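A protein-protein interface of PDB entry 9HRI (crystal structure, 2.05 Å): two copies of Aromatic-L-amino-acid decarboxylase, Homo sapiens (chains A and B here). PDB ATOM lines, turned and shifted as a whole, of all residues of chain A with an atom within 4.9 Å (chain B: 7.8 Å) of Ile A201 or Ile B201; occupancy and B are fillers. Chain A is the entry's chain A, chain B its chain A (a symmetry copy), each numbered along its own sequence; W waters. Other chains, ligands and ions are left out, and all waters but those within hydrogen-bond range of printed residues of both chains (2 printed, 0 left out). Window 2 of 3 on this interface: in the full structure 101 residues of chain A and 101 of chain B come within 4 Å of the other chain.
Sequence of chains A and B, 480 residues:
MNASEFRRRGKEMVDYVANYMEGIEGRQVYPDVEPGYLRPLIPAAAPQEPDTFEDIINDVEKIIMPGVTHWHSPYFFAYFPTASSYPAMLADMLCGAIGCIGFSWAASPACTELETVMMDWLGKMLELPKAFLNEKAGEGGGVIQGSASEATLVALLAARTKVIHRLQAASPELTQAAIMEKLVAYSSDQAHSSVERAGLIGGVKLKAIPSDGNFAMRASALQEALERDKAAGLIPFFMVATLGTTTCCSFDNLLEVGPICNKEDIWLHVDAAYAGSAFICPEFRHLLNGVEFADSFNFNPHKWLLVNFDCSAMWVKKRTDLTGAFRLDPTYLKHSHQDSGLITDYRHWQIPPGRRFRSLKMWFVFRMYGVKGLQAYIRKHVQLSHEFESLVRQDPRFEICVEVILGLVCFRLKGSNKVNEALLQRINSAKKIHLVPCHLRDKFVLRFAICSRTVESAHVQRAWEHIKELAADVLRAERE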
ATOM      1  N   LEU A 153      13.756  -9.185  -2.144  1.00  0.00           N
ATOM      2  CA  LEU A 153      13.861  -8.893  -0.719  1.00  0.00           C
ATOM      3  C   LEU A 153      14.792  -9.877  -0.023  1.00  0.00           C
ATOM      4  O   LEU A 153      15.630  -9.478   0.795  1.00  0.00           O
ATOM      5  CB  LEU A 153      12.477  -8.924  -0.068  1.00  0.00           C
ATOM      6  CG  LEU A 153      12.441  -8.776   1.457  1.00  0.00           C
ATOM      7  CD1 LEU A 153      13.172  -7.515   1.917  1.00  0.00           C
ATOM      8  CD2 LEU A 153      11.002  -8.804   1.964  1.00  0.00           C
ATOM      9  N   LEU A 157      18.240  -8.891   1.997  1.00  0.00           N
ATOM     10  CA  LEU A 157      18.466  -9.207   3.404  1.00  0.00           C
ATOM     11  C   LEU A 157      19.717 -10.055   3.585  1.00  0.00           C
ATOM     12  O   LEU A 157      20.467  -9.867   4.551  1.00  0.00           O
ATOM     13  CB  LEU A 157      17.243  -9.919   3.982  1.00  0.00           C
ATOM     14  CG  LEU A 157      15.973  -9.069   4.047  1.00  0.00           C
ATOM     15  CD1 LEU A 157      14.775  -9.931   4.408  1.00  0.00           C
ATOM     16  CD2 LEU A 157      16.136  -7.918   5.036  1.00  0.00           C
ATOM     17  N   ARG A 160      22.473  -7.656   3.174  1.00  0.00           N
ATOM     18  CA  ARG A 160      22.548  -6.791   4.346  1.00  0.00           C
ATOM     19  C   ARG A 160      23.230  -7.499   5.506  1.00  0.00           C
ATOM     20  O   ARG A 160      24.089  -6.917   6.179  1.00  0.00           O
ATOM     21  CB  ARG A 160      21.149  -6.324   4.751  1.00  0.00           C
ATOM     22  CG  ARG A 160      21.143  -5.129   5.692  1.00  0.00           C
ATOM     23  CD  ARG A 160      19.773  -4.913   6.315  1.00  0.00           C
ATOM     24  NE  ARG A 160      19.368  -6.034   7.152  1.00  0.00           N
ATOM     25  CZ  ARG A 160      18.161  -6.177   7.683  1.00  0.00           C
ATOM     26  NH1 ARG A 160      17.202  -5.292   7.469  1.00  0.00           N
ATOM     27  NH2 ARG A 160      17.911  -7.236   8.448  1.00  0.00           N
ATOM     28  N   ARG A 197      10.689  -1.269  -2.728  1.00  0.00           N
ATOM     29  CA  ARG A 197       9.989  -1.899  -1.614  1.00  0.00           C
ATOM     30  C   ARG A 197      10.957  -2.679  -0.733  1.00  0.00           C
ATOM     31  O   ARG A 197      10.907  -2.576   0.498  1.00  0.00           O
ATOM     32  CB  ARG A 197       8.880  -2.806  -2.155  1.00  0.00           C
ATOM     33  CG  ARG A 197       7.954  -3.416  -1.110  1.00  0.00           C
ATOM     34  CD  ARG A 197       7.187  -4.607  -1.702  1.00  0.00           C
ATOM     35  NE  ARG A 197       6.688  -5.548  -0.701  1.00  0.00           N
ATOM     36  CZ  ARG A 197       7.242  -6.721  -0.416  1.00  0.00           C
ATOM     37  NH1 ARG A 197       8.338  -7.137  -1.028  1.00  0.00           N
ATOM     38  NH2 ARG A 197       6.674  -7.500   0.501  1.00  0.00           N
ATOM     39  N   ALA A 198      11.863  -3.442  -1.350  1.00  0.00           N
ATOM     40  CA  ALA A 198      12.836  -4.210  -0.580  1.00  0.00           C
ATOM     41  C   ALA A 198      13.769  -3.296   0.203  1.00  0.00           C
ATOM     42  O   ALA A 198      14.119  -3.591   1.352  1.00  0.00           O
ATOM     43  CB  ALA A 198      13.634  -5.126  -1.508  1.00  0.00           C
ATOM     44  N   GLY A 199      14.185  -2.182  -0.402  1.00  0.00           N
ATOM     45  CA  GLY A 199      15.035  -1.242   0.308  1.00  0.00           C
ATOM     46  C   GLY A 199      14.338  -0.607   1.496  1.00  0.00           C
ATOM     47  O   GLY A 199      14.945  -0.417   2.554  1.00  0.00           O
ATOM     48  N   LEU A 200      13.055  -0.272   1.341  1.00  0.00           N
ATOM     49  CA  LEU A 200      12.307   0.300   2.456  1.00  0.00           C
ATOM     50  C   LEU A 200      12.126  -0.717   3.576  1.00  0.00           C
ATOM     51  O   LEU A 200      12.299  -0.385   4.755  1.00  0.00           O
ATOM     52  CB  LEU A 200      10.950   0.813   1.973  1.00  0.00           C
ATOM     53  CG  LEU A 200      10.985   2.039   1.056  1.00  0.00           C
ATOM     54  CD1 LEU A 200       9.637   2.252   0.381  1.00  0.00           C
ATOM     55  CD2 LEU A 200      11.407   3.275   1.837  1.00  0.00           C
ATOM     56  N   ILE A 201      11.776  -1.957   3.227  1.00  0.00           N
ATOM     57  CA  ILE A 201      11.652  -3.010   4.233  1.00  0.00           C
ATOM     58  C   ILE A 201      12.985  -3.222   4.940  1.00  0.00           C
ATOM     59  O   ILE A 201      13.054  -3.267   6.174  1.00  0.00           O
ATOM     60  CB  ILE A 201      11.148  -4.315   3.589  1.00  0.00           C
ATOM     61  CG1 ILE A 201       9.703  -4.166   3.108  1.00  0.00           C
ATOM     62  CG2 ILE A 201      11.252  -5.470   4.577  1.00  0.00           C
ATOM     63  CD1 ILE A 201       9.242  -5.306   2.229  1.00  0.00           C
ATOM     64  N   GLY A 202      14.065  -3.350   4.165  1.00  0.00           N
ATOM     65  CA  GLY A 202      15.379  -3.592   4.732  1.00  0.00           C
ATOM     66  C   GLY A 202      15.962  -2.408   5.474  1.00  0.00           C
ATOM     67  O   GLY A 202      16.928  -2.580   6.225  1.00  0.00           O
ATOM     68  N   GLY A 203      15.404  -1.214   5.284  1.00  0.00           N
ATOM     69  CA  GLY A 203      15.896  -0.036   5.974  1.00  0.00           C
ATOM     70  C   GLY A 203      17.171   0.548   5.415  1.00  0.00           C
ATOM     71  O   GLY A 203      17.958   1.128   6.168  1.00  0.00           O
ATOM     72  N   SER B 149       3.021 -15.287   9.587  1.00  0.00           N
ATOM     73  CA  SER B 149       4.374 -14.747   9.634  1.00  0.00           C
ATOM     74  C   SER B 149       4.467 -13.454   8.840  1.00  0.00           C
ATOM     75  O   SER B 149       5.091 -12.482   9.286  1.00  0.00           O
ATOM     76  CB  SER B 149       5.367 -15.772   9.087  1.00  0.00           C
ATOM     77  OG  SER B 149       5.340 -16.959   9.857  1.00  0.00           O
ATOM     78  N   LEU B 153       5.042  -9.564  10.250  1.00  0.00           N
ATOM     79  CA  LEU B 153       6.041  -8.696   9.637  1.00  0.00           C
ATOM     80  C   LEU B 153       5.419  -7.388   9.168  1.00  0.00           C
ATOM     81  O   LEU B 153       5.986  -6.310   9.383  1.00  0.00           O
ATOM     82  CB  LEU B 153       6.716  -9.411   8.465  1.00  0.00           C
ATOM     83  CG  LEU B 153       7.690  -8.572   7.628  1.00  0.00           C
ATOM     84  CD1 LEU B 153       8.769  -7.930   8.500  1.00  0.00           C
ATOM     85  CD2 LEU B 153       8.300  -9.415   6.512  1.00  0.00           C
ATOM     86  N   VAL B 154       4.252  -7.464   8.521  1.00  0.00           N
ATOM     87  CA  VAL B 154       3.587  -6.261   8.030  1.00  0.00           C
ATOM     88  C   VAL B 154       3.245  -5.330   9.186  1.00  0.00           C
ATOM     89  O   VAL B 154       3.426  -4.108   9.094  1.00  0.00           O
ATOM     90  CB  VAL B 154       2.335  -6.643   7.215  1.00  0.00           C
ATOM     91  CG1 VAL B 154       1.436  -5.432   7.026  1.00  0.00           C
ATOM     92  CG2 VAL B 154       2.737  -7.231   5.871  1.00  0.00           C
ATOM     93  N   LEU B 156       4.783  -5.170  12.107  1.00  0.00           N
ATOM     94  CA  LEU B 156       6.019  -4.614  12.650  1.00  0.00           C
ATOM     95  C   LEU B 156       6.528  -3.466  11.790  1.00  0.00           C
ATOM     96  O   LEU B 156       6.970  -2.435  12.312  1.00  0.00           O
ATOM     97  CB  LEU B 156       7.082  -5.708  12.771  1.00  0.00           C
ATOM     98  CG  LEU B 156       8.392  -5.329  13.475  1.00  0.00           C
ATOM     99  CD1 LEU B 156       8.905  -6.503  14.299  1.00  0.00           C
ATOM    100  CD2 LEU B 156       9.464  -4.862  12.492  1.00  0.00           C
ATOM    101  N   LEU B 157       6.483  -3.629  10.466  1.00  0.00           N
ATOM    102  CA  LEU B 157       6.959  -2.576   9.575  1.00  0.00           C
ATOM    103  C   LEU B 157       6.080  -1.336   9.667  1.00  0.00           C
ATOM    104  O   LEU B 157       6.583  -0.207   9.623  1.00  0.00           O
ATOM    105  CB  LEU B 157       7.013  -3.093   8.137  1.00  0.00           C
ATOM    106  CG  LEU B 157       8.035  -4.204   7.890  1.00  0.00           C
ATOM    107  CD1 LEU B 157       7.843  -4.803   6.507  1.00  0.00           C
ATOM    108  CD2 LEU B 157       9.459  -3.686   8.068  1.00  0.00           C
ATOM    109  N   ARG B 160       7.086   0.218  12.844  1.00  0.00           N
ATOM    110  CA  ARG B 160       8.407   0.820  12.699  1.00  0.00           C
ATOM    111  C   ARG B 160       8.322   2.158  11.977  1.00  0.00           C
ATOM    112  O   ARG B 160       8.950   3.136  12.397  1.00  0.00           O
ATOM    113  CB  ARG B 160       9.344  -0.132  11.954  1.00  0.00           C
ATOM    114  CG  ARG B 160      10.819   0.216  12.093  1.00  0.00           C
ATOM    115  CD  ARG B 160      11.671  -0.544  11.089  1.00  0.00           C
ATOM    116  NE  ARG B 160      11.344  -0.191   9.713  1.00  0.00           N
ATOM    117  CZ  ARG B 160      11.819  -0.818   8.645  1.00  0.00           C
ATOM    118  NH1 ARG B 160      12.638  -1.850   8.756  1.00  0.00           N
ATOM    119  NH2 ARG B 160      11.464  -0.395   7.435  1.00  0.00           N
ATOM    120  N   GLN B 176      16.918   8.041  10.841  1.00  0.00           N
ATOM    121  CA  GLN B 176      16.201   6.779  10.981  1.00  0.00           C
ATOM    122  C   GLN B 176      17.054   5.744  11.706  1.00  0.00           C
ATOM    123  O   GLN B 176      16.550   5.005  12.560  1.00  0.00           O
ATOM    124  CB  GLN B 176      15.764   6.261   9.609  1.00  0.00           C
ATOM    125  CG  GLN B 176      15.475   4.761   9.568  1.00  0.00           C
ATOM    126  CD  GLN B 176      14.457   4.382   8.503  1.00  0.00           C
ATOM    127  OE1 GLN B 176      13.744   5.238   7.978  1.00  0.00           O
ATOM    128  NE2 GLN B 176      14.386   3.093   8.179  1.00  0.00           N
ATOM    129  N   MET B 180      16.736   3.465  15.086  1.00  0.00           N
ATOM    130  CA  MET B 180      16.648   2.021  14.878  1.00  0.00           C
ATOM    131  C   MET B 180      17.290   1.240  16.019  1.00  0.00           C
ATOM    132  O   MET B 180      16.713   0.268  16.519  1.00  0.00           O
ATOM    133  CB  MET B 180      17.300   1.648  13.545  1.00  0.00           C
ATOM    134  CG  MET B 180      16.435   1.926  12.339  1.00  0.00           C
ATOM    135  SD  MET B 180      14.855   1.089  12.474  1.00  0.00           S
ATOM    136  CE  MET B 180      15.356  -0.588  12.100  1.00  0.00           C
ATOM    137  N   SER B 194       8.112 -16.668  14.134  1.00  0.00           N
ATOM    138  CA  SER B 194       7.869 -15.618  13.149  1.00  0.00           C
ATOM    139  C   SER B 194       8.095 -14.229  13.732  1.00  0.00           C
ATOM    140  O   SER B 194       8.447 -13.297  12.998  1.00  0.00           O
ATOM    141  CB  SER B 194       6.445 -15.732  12.608  1.00  0.00           C
ATOM    142  OG  SER B 194       5.502 -15.761  13.667  1.00  0.00           O
ATOM    143  N   VAL B 195       7.892 -14.066  15.040  1.00  0.00           N
ATOM    144  CA  VAL B 195       8.133 -12.772  15.672  1.00  0.00           C
ATOM    145  C   VAL B 195       9.612 -12.417  15.600  1.00  0.00           C
ATOM    146  O   VAL B 195       9.983 -11.311  15.188  1.00  0.00           O
ATOM    147  CB  VAL B 195       7.624 -12.779  17.124  1.00  0.00           C
ATOM    148  CG1 VAL B 195       7.745 -11.392  17.738  1.00  0.00           C
ATOM    149  CG2 VAL B 195       6.184 -13.270  17.180  1.00  0.00           C
ATOM    150  N   GLU B 196      10.478 -13.351  16.001  1.00  0.00           N
ATOM    151  CA  GLU B 196      11.917 -13.128  15.892  1.00  0.00           C
ATOM    152  C   GLU B 196      12.322 -12.874  14.447  1.00  0.00           C
ATOM    153  O   GLU B 196      13.136 -11.984  14.168  1.00  0.00           O
ATOM    154  CB  GLU B 196      12.675 -14.329  16.460  1.00  0.00           C
ATOM    155  CG  GLU B 196      14.188 -14.245  16.322  1.00  0.00           C
ATOM    156  CD  GLU B 196      14.898 -15.445  16.923  1.00  0.00           C
ATOM    157  OE1 GLU B 196      14.331 -16.085  17.833  1.00  0.00           O
ATOM    158  OE2 GLU B 196      16.027 -15.746  16.483  1.00  0.00           O
ATOM    159  N   ARG B 197      11.757 -13.646  13.516  1.00  0.00           N
ATOM    160  CA  ARG B 197      12.046 -13.447  12.100  1.00  0.00           C
ATOM    161  C   ARG B 197      11.680 -12.036  11.662  1.00  0.00           C
ATOM    162  O   ARG B 197      12.458 -11.372  10.966  1.00  0.00           O
ATOM    163  CB  ARG B 197      11.296 -14.496  11.274  1.00  0.00           C
ATOM    164  CG  ARG B 197      11.617 -14.521   9.784  1.00  0.00           C
ATOM    165  CD  ARG B 197      10.529 -15.281   9.013  1.00  0.00           C
ATOM    166  NE  ARG B 197      10.459 -14.937   7.594  1.00  0.00           N
ATOM    167  CZ  ARG B 197       9.551 -14.137   7.048  1.00  0.00           C
ATOM    168  NH1 ARG B 197       8.612 -13.555   7.776  1.00  0.00           N
ATOM    169  NH2 ARG B 197       9.579 -13.925   5.734  1.00  0.00           N
ATOM    170  N   ALA B 198      10.509 -11.551  12.084  1.00  0.00           N
ATOM    171  CA  ALA B 198      10.089 -10.201  11.721  1.00  0.00           C
ATOM    172  C   ALA B 198      11.024  -9.152  12.311  1.00  0.00           C
ATOM    173  O   ALA B 198      11.343  -8.154  11.654  1.00  0.00           O
ATOM    174  CB  ALA B 198       8.651  -9.958  12.179  1.00  0.00           C
ATOM    175  N   GLY B 199      11.471  -9.359  13.550  1.00  0.00           N
ATOM    176  CA  GLY B 199      12.406  -8.423  14.153  1.00  0.00           C
ATOM    177  C   GLY B 199      13.740  -8.387  13.434  1.00  0.00           C
ATOM    178  O   GLY B 199      14.331  -7.317  13.256  1.00  0.00           O
ATOM    179  N   LEU B 200      14.234  -9.552  13.008  1.00  0.00           N
ATOM    180  CA  LEU B 200      15.490  -9.590  12.267  1.00  0.00           C
ATOM    181  C   LEU B 200      15.349  -8.911  10.910  1.00  0.00           C
ATOM    182  O   LEU B 200      16.226  -8.140  10.502  1.00  0.00           O
ATOM    183  CB  LEU B 200      15.961 -11.036  12.099  1.00  0.00           C
ATOM    184  CG  LEU B 200      16.416 -11.745  13.375  1.00  0.00           C
ATOM    185  CD1 LEU B 200      16.539 -13.245  13.150  1.00  0.00           C
ATOM    186  CD2 LEU B 200      17.729 -11.158  13.870  1.00  0.00           C
ATOM    187  N   ILE B 201      14.254  -9.190  10.197  1.00  0.00           N
ATOM    188  CA  ILE B 201      14.007  -8.528   8.919  1.00  0.00           C
ATOM    189  C   ILE B 201      13.907  -7.020   9.117  1.00  0.00           C
ATOM    190  O   ILE B 201      14.540  -6.237   8.400  1.00  0.00           O
ATOM    191  CB  ILE B 201      12.735  -9.088   8.256  1.00  0.00           C
ATOM    192  CG1 ILE B 201      12.939 -10.542   7.825  1.00  0.00           C
ATOM    193  CG2 ILE B 201      12.341  -8.238   7.054  1.00  0.00           C
ATOM    194  CD1 ILE B 201      11.658 -11.235   7.422  1.00  0.00           C
ATOM    195  N   GLY B 202      13.110  -6.594  10.100  1.00  0.00           N
ATOM    196  CA  GLY B 202      12.913  -5.178  10.354  1.00  0.00           C
ATOM    197  C   GLY B 202      14.124  -4.475  10.931  1.00  0.00           C
ATOM    198  O   GLY B 202      14.168  -3.242  10.923  1.00  0.00           O
ATOM    199  N   GLY B 203      15.103  -5.227  11.432  1.00  0.00           N
ATOM    200  CA  GLY B 203      16.302  -4.627  11.984  1.00  0.00           C
ATOM    201  C   GLY B 203      16.145  -4.037  13.365  1.00  0.00           C
ATOM    202  O   GLY B 203      16.833  -3.067  13.697  1.00  0.00           O
ATOM    203  N   VAL B 204      15.262  -4.598  14.190  1.00  0.00           N
ATOM    204  CA  VAL B 204      15.008  -4.087  15.530  1.00  0.00           C
ATOM    205  C   VAL B 204      15.267  -5.191  16.545  1.00  0.00           C
ATOM    206  O   VAL B 204      15.262  -6.383  16.226  1.00  0.00           O
ATOM    207  CB  VAL B 204      13.575  -3.538  15.685  1.00  0.00           C
ATOM    208  CG1 VAL B 204      13.324  -2.414  14.696  1.00  0.00           C
ATOM    209  CG2 VAL B 204      12.551  -4.652  15.492  1.00  0.00           C
HETATM  210  O   HOH W   1      13.195   2.351   5.666  1.00  0.00           O
HETATM  211  O   HOH W   2      17.395   1.856   8.742  1.00  0.00           O
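The guanidinium group (NH1) of Arg A160 sits at hydrogen-bond distance from the backbone carbonyl oxygen (O) of Ile B201, 3.0 Å away. NH2 of Arg A160 lies within hydrogen-bond range of O of Leu B200. O of Leu A200 is in hydrogen-bond range of NH2 of Arg B160 (2.8 Å). The backbone carbonyl oxygen (O) of Ile A201 is in hydrogen-bond range of the guanidinium group (NH1) of Arg B160 (3.0 Å).
The guanidinium group (NH1) of Arg A160 is in hydrogen-bond range of the backbone carbonyl oxygen (O) of Gly A202, 3.0 Å away. O of Gly B202 is in hydrogen-bond range of NH1 of Arg B160 (3.0 Å).
Among the printed residues, pairs that only touch across the chains: Ile A201 with Ile B201 (3.9 Å), Ile A201 with Leu B157 (3.9 Å) and Leu A157 with Ile B201 (3.9 Å).
Of the printed residues of chain B, Leu A200 touches Arg B160. Ile A201 touches three residues of chain B. Of the printed residues of chain A, Arg B160 touches Leu A200 (2.8 Å) and Ile A201 (3.0 Å). Ile B201 touches just these residues of chain A: Leu A157 (3.9 Å), Arg A160 (3.0 Å) and Ile A201 (3.9 Å). The nearest residue of chain B that does not touch Ile A201 is Gly B202 (4.6 Å). The nearest printed residue of chain B that does not touch Arg A160 is Gly B203 (4.5 Å).
Printed residues of chain B that touch a printed residue of chain A: Leu B157, Arg B160, Leu B200 and Ile B201. Hydrophobic or aromatic side chains of chain B within 4 Å of the printed part of chain A: Leu B157 and Ile B201. Along chain B the printed residues that touch a printed residue of chain A span positions 157 to 201. Of the 10 printed residues of chain A, 4 touch a printed residue of chain B. Hydrophobic or aromatic side chains of chain A that line the printed part of chain B: Leu A157 and Ile A201. Among the printed residues, no Asp or Glu carboxylate lies within 4 Å of a Lys or Arg side-chain nitrogen of the other chain.
Leu A157 touches Ile B201, and with the chains exchanged Ile A201 touches Leu B157. Arg A160 touches Leu B200, and with the chains exchanged Leu A200 touches Arg B160. Arg A160 touches Ile B201, and with the chains exchanged Ile A201 touches Arg B160. Ile A201 touches its own counterpart, Ile B201. Positions printed for both chains: 153, 157, 160, 197, 198, 199, 200, 201, 202 and 203.
Water W2 bridges the backbone carbonyl oxygen of Gly A203 and the side-chain amide nitrogen of Gln B176. Water W1 lies within hydrogen-bond range of NE2 of Gln B176 and O of Leu A200.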
